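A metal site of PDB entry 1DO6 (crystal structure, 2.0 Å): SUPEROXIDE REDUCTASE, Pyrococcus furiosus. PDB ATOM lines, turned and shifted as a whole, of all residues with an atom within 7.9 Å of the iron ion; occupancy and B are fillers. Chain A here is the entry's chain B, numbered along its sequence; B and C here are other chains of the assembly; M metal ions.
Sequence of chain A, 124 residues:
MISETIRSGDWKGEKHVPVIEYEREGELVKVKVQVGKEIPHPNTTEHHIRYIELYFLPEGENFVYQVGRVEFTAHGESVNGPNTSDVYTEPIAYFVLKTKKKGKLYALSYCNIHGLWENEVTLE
O of His 114 is in hydrogen-bond range of NE1 of Trp 117, 2.8 Å away.
A ring nitrogen (NE2) of His 16 sits close to the side-chain amino group (NZ) of Lys 15, at 3.2 Å.
ND1 of His 16 lies within hydrogen-bond range of OE2 of Glu 14, at 3.0 Å.
The side-chain sulfur of Cys 111 lies close to the backbone NH of Ile 113 (3.7 Å).
Merely in contact with the iron ion: Lys 15 (3.5 Å).
Of the 18 residues printed, 6 come within 4 Å of the iron ion.
Along chain A the residues within 4 Å of the iron ion span positions 15 to 114.
The nearest printed residue that does not touch the iron ion is Ile 113 (4.5 Å).
The iron ion is bound by a ring nitrogen (ND1) of His 114, 2.0 Å away.
NE2 of His 16 is bound to the iron ion, at 2.1 Å.
A ring nitrogen (NE2) of His 47 is bound to the iron ion (2.2 Å).
NE2 of His 41 binds the iron ion, 2.2 Å away.
SG of Cys 111 is bound to the iron ion, at 2.3 Å.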
ATOM      1  N   GLU A  14      -6.876 -10.674  -2.240  1.00  0.00           N
ATOM      2  CA  GLU A  14      -6.631 -10.902  -0.816  1.00  0.00           C
ATOM      3  C   GLU A  14      -6.024 -12.292  -0.594  1.00  0.00           C
ATOM      4  O   GLU A  14      -6.696 -13.311  -0.769  1.00  0.00           O
ATOM      5  CB  GLU A  14      -7.937 -10.777  -0.016  1.00  0.00           C
ATOM      6  CG  GLU A  14      -7.872  -9.742   1.108  1.00  0.00           C
ATOM      7  CD  GLU A  14      -6.755 -10.004   2.147  1.00  0.00           C
ATOM      8  OE1 GLU A  14      -6.468  -9.082   2.935  1.00  0.00           O
ATOM      9  OE2 GLU A  14      -6.176 -11.108   2.170  1.00  0.00           O
ATOM     10  N   LYS A  15      -4.749 -12.287  -0.186  1.00  0.00           N
ATOM     11  CA  LYS A  15      -3.968 -13.489   0.066  1.00  0.00           C
ATOM     12  C   LYS A  15      -4.516 -14.473   1.109  1.00  0.00           C
ATOM     13  O   LYS A  15      -4.008 -15.578   1.231  1.00  0.00           O
ATOM     14  CB  LYS A  15      -2.534 -13.099   0.468  1.00  0.00           C
ATOM     15  CG  LYS A  15      -2.462 -11.966   1.505  1.00  0.00           C
ATOM     16  CD  LYS A  15      -1.087 -11.890   2.184  1.00  0.00           C
ATOM     17  CE  LYS A  15      -1.127 -11.014   3.434  1.00  0.00           C
ATOM     18  NZ  LYS A  15      -1.016 -11.804   4.712  1.00  0.00           N
ATOM     19  N   HIS A  16      -5.538 -14.092   1.860  1.00  0.00           N
ATOM     20  CA  HIS A  16      -6.074 -14.979   2.880  1.00  0.00           C
ATOM     21  C   HIS A  16      -7.242 -15.867   2.454  1.00  0.00           C
ATOM     22  O   HIS A  16      -7.522 -16.893   3.098  1.00  0.00           O
ATOM     23  CB  HIS A  16      -6.510 -14.170   4.102  1.00  0.00           C
ATOM     24  CG  HIS A  16      -5.377 -13.526   4.829  1.00  0.00           C
ATOM     25  ND1 HIS A  16      -5.113 -12.167   4.792  1.00  0.00           N
ATOM     26  CD2 HIS A  16      -4.458 -14.054   5.668  1.00  0.00           C
ATOM     27  CE1 HIS A  16      -4.054 -11.922   5.589  1.00  0.00           C
ATOM     28  NE2 HIS A  16      -3.618 -13.036   6.142  1.00  0.00           N
ATOM     29  N   VAL A  35      -4.507 -21.640   0.269  1.00  0.00           N
ATOM     30  CA  VAL A  35      -4.444 -20.225   0.582  1.00  0.00           C
ATOM     31  C   VAL A  35      -3.146 -19.670  -0.031  1.00  0.00           C
ATOM     32  O   VAL A  35      -2.091 -20.275   0.125  1.00  0.00           O
ATOM     33  CB  VAL A  35      -4.402 -19.986   2.080  1.00  0.00           C
ATOM     34  CG1 VAL A  35      -4.123 -18.504   2.338  1.00  0.00           C
ATOM     35  CG2 VAL A  35      -5.714 -20.411   2.709  1.00  0.00           C
ATOM     36  N   HIS A  41       1.056 -16.632   0.836  1.00  0.00           N
ATOM     37  CA  HIS A  41       0.863 -16.090   2.168  1.00  0.00           C
ATOM     38  C   HIS A  41       2.105 -16.460   2.962  1.00  0.00           C
ATOM     39  O   HIS A  41       2.695 -17.519   2.753  1.00  0.00           O
ATOM     40  CB  HIS A  41      -0.390 -16.651   2.834  1.00  0.00           C
ATOM     41  CG  HIS A  41      -0.605 -16.162   4.232  1.00  0.00           C
ATOM     42  ND1 HIS A  41       0.098 -16.610   5.330  1.00  0.00           N
ATOM     43  CD2 HIS A  41      -1.473 -15.227   4.710  1.00  0.00           C
ATOM     44  CE1 HIS A  41      -0.351 -15.959   6.419  1.00  0.00           C
ATOM     45  NE2 HIS A  41      -1.313 -15.094   6.097  1.00  0.00           N
ATOM     46  N   PRO A  42       2.528 -15.587   3.873  1.00  0.00           N
ATOM     47  CA  PRO A  42       3.733 -15.967   4.629  1.00  0.00           C
ATOM     48  C   PRO A  42       3.552 -17.265   5.413  1.00  0.00           C
ATOM     49  O   PRO A  42       2.443 -17.631   5.830  1.00  0.00           O
ATOM     50  CB  PRO A  42       3.951 -14.784   5.577  1.00  0.00           C
ATOM     51  CG  PRO A  42       3.172 -13.628   4.969  1.00  0.00           C
ATOM     52  CD  PRO A  42       2.006 -14.262   4.263  1.00  0.00           C
ATOM     53  N   HIS A  47       3.860 -15.851  11.831  1.00  0.00           N
ATOM     54  CA  HIS A  47       2.746 -15.551  10.953  1.00  0.00           C
ATOM     55  C   HIS A  47       2.548 -16.663   9.957  1.00  0.00           C
ATOM     56  O   HIS A  47       3.373 -16.858   9.057  1.00  0.00           O
ATOM     57  CB  HIS A  47       3.051 -14.249  10.208  1.00  0.00           C
ATOM     58  CG  HIS A  47       1.935 -13.779   9.333  1.00  0.00           C
ATOM     59  ND1 HIS A  47       2.088 -12.842   8.331  1.00  0.00           N
ATOM     60  CD2 HIS A  47       0.627 -14.143   9.319  1.00  0.00           C
ATOM     61  CE1 HIS A  47       0.880 -12.676   7.755  1.00  0.00           C
ATOM     62  NE2 HIS A  47      -0.023 -13.447   8.338  1.00  0.00           N
ATOM     63  N   HIS A  48       1.441 -17.404  10.093  1.00  0.00           N
ATOM     64  CA  HIS A  48       1.214 -18.528   9.196  1.00  0.00           C
ATOM     65  C   HIS A  48      -0.250 -18.964   9.179  1.00  0.00           C
ATOM     66  O   HIS A  48      -1.006 -18.618  10.081  1.00  0.00           O
ATOM     67  CB  HIS A  48       2.052 -19.696   9.685  1.00  0.00           C
ATOM     68  CG  HIS A  48       1.844 -20.008  11.143  1.00  0.00           C
ATOM     69  ND1 HIS A  48       2.764 -19.674  12.111  1.00  0.00           N
ATOM     70  CD2 HIS A  48       0.813 -20.595  11.791  1.00  0.00           C
ATOM     71  CE1 HIS A  48       2.309 -20.051  13.294  1.00  0.00           C
ATOM     72  NE2 HIS A  48       1.120 -20.606  13.131  1.00  0.00           N
ATOM     73  N   ILE A  49      -0.617 -19.759   8.175  1.00  0.00           N
ATOM     74  CA  ILE A  49      -1.987 -20.306   8.084  1.00  0.00           C
ATOM     75  C   ILE A  49      -2.015 -21.565   8.969  1.00  0.00           C
ATOM     76  O   ILE A  49      -1.209 -22.477   8.775  1.00  0.00           O
ATOM     77  CB  ILE A  49      -2.324 -20.709   6.638  1.00  0.00           C
ATOM     78  CG1 ILE A  49      -2.301 -19.459   5.731  1.00  0.00           C
ATOM     79  CG2 ILE A  49      -3.702 -21.445   6.617  1.00  0.00           C
ATOM     80  CD1 ILE A  49      -3.125 -18.292   6.286  1.00  0.00           C
ATOM     81  N   TYR A 110      -7.895 -20.156   8.785  1.00  0.00           N
ATOM     82  CA  TYR A 110      -7.500 -19.338   9.927  1.00  0.00           C
ATOM     83  C   TYR A 110      -6.018 -18.952   9.862  1.00  0.00           C
ATOM     84  O   TYR A 110      -5.158 -19.826   9.799  1.00  0.00           O
ATOM     85  CB  TYR A 110      -7.759 -20.095  11.217  1.00  0.00           C
ATOM     86  CG  TYR A 110      -7.355 -19.333  12.474  1.00  0.00           C
ATOM     87  CD1 TYR A 110      -8.065 -18.207  12.905  1.00  0.00           C
ATOM     88  CD2 TYR A 110      -6.261 -19.750  13.252  1.00  0.00           C
ATOM     89  CE1 TYR A 110      -7.713 -17.510  14.057  1.00  0.00           C
ATOM     90  CE2 TYR A 110      -5.898 -19.054  14.417  1.00  0.00           C
ATOM     91  CZ  TYR A 110      -6.621 -17.936  14.805  1.00  0.00           C
ATOM     92  OH  TYR A 110      -6.235 -17.209  15.908  1.00  0.00           O
ATOM     93  N   CYS A 111      -5.746 -17.639   9.897  1.00  0.00           N
ATOM     94  CA  CYS A 111      -4.370 -17.133   9.882  1.00  0.00           C
ATOM     95  C   CYS A 111      -4.125 -16.852  11.348  1.00  0.00           C
ATOM     96  O   CYS A 111      -5.017 -16.323  12.011  1.00  0.00           O
ATOM     97  CB  CYS A 111      -4.290 -15.854   9.037  1.00  0.00           C
ATOM     98  SG  CYS A 111      -2.719 -14.959   9.273  1.00  0.00           S
ATOM     99  N   ASN A 112      -2.968 -17.208  11.881  1.00  0.00           N
ATOM    100  CA  ASN A 112      -2.763 -16.986  13.316  1.00  0.00           C
ATOM    101  C   ASN A 112      -2.857 -15.528  13.803  1.00  0.00           C
ATOM    102  O   ASN A 112      -3.075 -15.310  14.996  1.00  0.00           O
ATOM    103  CB  ASN A 112      -1.447 -17.634  13.798  1.00  0.00           C
ATOM    104  CG  ASN A 112      -0.207 -16.879  13.285  1.00  0.00           C
ATOM    105  OD1 ASN A 112      -0.203 -16.377  12.185  1.00  0.00           O
ATOM    106  ND2 ASN A 112       0.854 -16.828  14.114  1.00  0.00           N
ATOM    107  N   ILE A 113      -2.721 -14.551  12.926  1.00  0.00           N
ATOM    108  CA  ILE A 113      -2.817 -13.150  13.350  1.00  0.00           C
ATOM    109  C   ILE A 113      -3.860 -12.366  12.566  1.00  0.00           C
ATOM    110  O   ILE A 113      -4.157 -11.212  12.900  1.00  0.00           O
ATOM    111  CB  ILE A 113      -1.448 -12.370  13.216  1.00  0.00           C
ATOM    112  CG1 ILE A 113      -0.986 -12.377  11.755  1.00  0.00           C
ATOM    113  CG2 ILE A 113      -0.391 -12.981  14.142  1.00  0.00           C
ATOM    114  CD1 ILE A 113       0.227 -11.442  11.486  1.00  0.00           C
ATOM    115  N   HIS A 114      -4.425 -12.977  11.527  1.00  0.00           N
ATOM    116  CA  HIS A 114      -5.410 -12.293  10.699  1.00  0.00           C
ATOM    117  C   HIS A 114      -6.839 -12.865  10.723  1.00  0.00           C
ATOM    118  O   HIS A 114      -7.621 -12.627   9.807  1.00  0.00           O
ATOM    119  CB  HIS A 114      -4.908 -12.218   9.265  1.00  0.00           C
ATOM    120  CG  HIS A 114      -3.700 -11.347   9.078  1.00  0.00           C
ATOM    121  ND1 HIS A 114      -2.599 -11.780   8.354  1.00  0.00           N
ATOM    122  CD2 HIS A 114      -3.484 -10.079   9.513  1.00  0.00           C
ATOM    123  CE1 HIS A 114      -1.746 -10.766   8.353  1.00  0.00           C
ATOM    124  NE2 HIS A 114      -2.227  -9.711   9.046  1.00  0.00           N
ATOM    125  N   GLY A 115      -7.165 -13.601  11.776  1.00  0.00           N
ATOM    126  CA  GLY A 115      -8.500 -14.160  11.934  1.00  0.00           C
ATOM    127  C   GLY A 115      -8.983 -15.182  10.930  1.00  0.00           C
ATOM    128  O   GLY A 115      -8.206 -15.816  10.195  1.00  0.00           O
ATOM    129  N   TRP A 117     -11.225 -16.657   7.661  1.00  0.00           N
ATOM    130  CA  TRP A 117     -11.526 -16.347   6.263  1.00  0.00           C
ATOM    131  C   TRP A 117     -12.388 -17.458   5.685  1.00  0.00           C
ATOM    132  O   TRP A 117     -12.206 -18.621   6.031  1.00  0.00           O
ATOM    133  CB  TRP A 117     -10.227 -16.238   5.453  1.00  0.00           C
ATOM    134  CG  TRP A 117      -9.411 -15.074   5.939  1.00  0.00           C
ATOM    135  CD1 TRP A 117      -8.631 -15.039   7.080  1.00  0.00           C
ATOM    136  CD2 TRP A 117      -9.407 -13.756   5.413  1.00  0.00           C
ATOM    137  NE1 TRP A 117      -8.163 -13.747   7.288  1.00  0.00           N
ATOM    138  CE2 TRP A 117      -8.627 -12.945   6.281  1.00  0.00           C
ATOM    139  CE3 TRP A 117     -10.005 -13.169   4.285  1.00  0.00           C
ATOM    140  CZ2 TRP A 117      -8.429 -11.577   6.050  1.00  0.00           C
ATOM    141  CZ3 TRP A 117      -9.799 -11.795   4.055  1.00  0.00           C
ATOM    142  CH2 TRP A 117      -9.015 -11.028   4.931  1.00  0.00           C
ATOM    143  N   VAL B  79      -0.554  -8.878  14.919  1.00  0.00           N
ATOM    144  CA  VAL B  79      -0.011  -8.097  13.814  1.00  0.00           C
ATOM    145  C   VAL B  79       1.133  -7.191  14.346  1.00  0.00           C
ATOM    146  O   VAL B  79       1.899  -6.650  13.561  1.00  0.00           O
ATOM    147  CB  VAL B  79      -1.085  -7.170  13.207  1.00  0.00           C
ATOM    148  CG1 VAL B  79      -2.074  -7.994  12.355  1.00  0.00           C
ATOM    149  CG2 VAL B  79      -1.810  -6.448  14.324  1.00  0.00           C
ATOM    150  N   PHE C  63      -9.058  -8.555  14.618  1.00  0.00           N
ATOM    151  CA  PHE C  63      -8.899  -9.960  14.293  1.00  0.00           C
ATOM    152  C   PHE C  63      -9.198 -10.868  15.443  1.00  0.00           C
ATOM    153  O   PHE C  63      -8.730 -10.662  16.577  1.00  0.00           O
ATOM    154  CB  PHE C  63      -7.492 -10.199  13.752  1.00  0.00           C
ATOM    155  CG  PHE C  63      -7.146  -9.304  12.584  1.00  0.00           C
ATOM    156  CD1 PHE C  63      -6.291  -8.214  12.748  1.00  0.00           C
ATOM    157  CD2 PHE C  63      -7.688  -9.557  11.326  1.00  0.00           C
ATOM    158  CE1 PHE C  63      -5.979  -7.375  11.664  1.00  0.00           C
ATOM    159  CE2 PHE C  63      -7.377  -8.733  10.234  1.00  0.00           C
ATOM    160  CZ  PHE C  63      -6.514  -7.637  10.399  1.00  0.00           C
HETATM  161 FE    FE M   1      -2.057 -13.568   7.514  1.00  0.00          FE
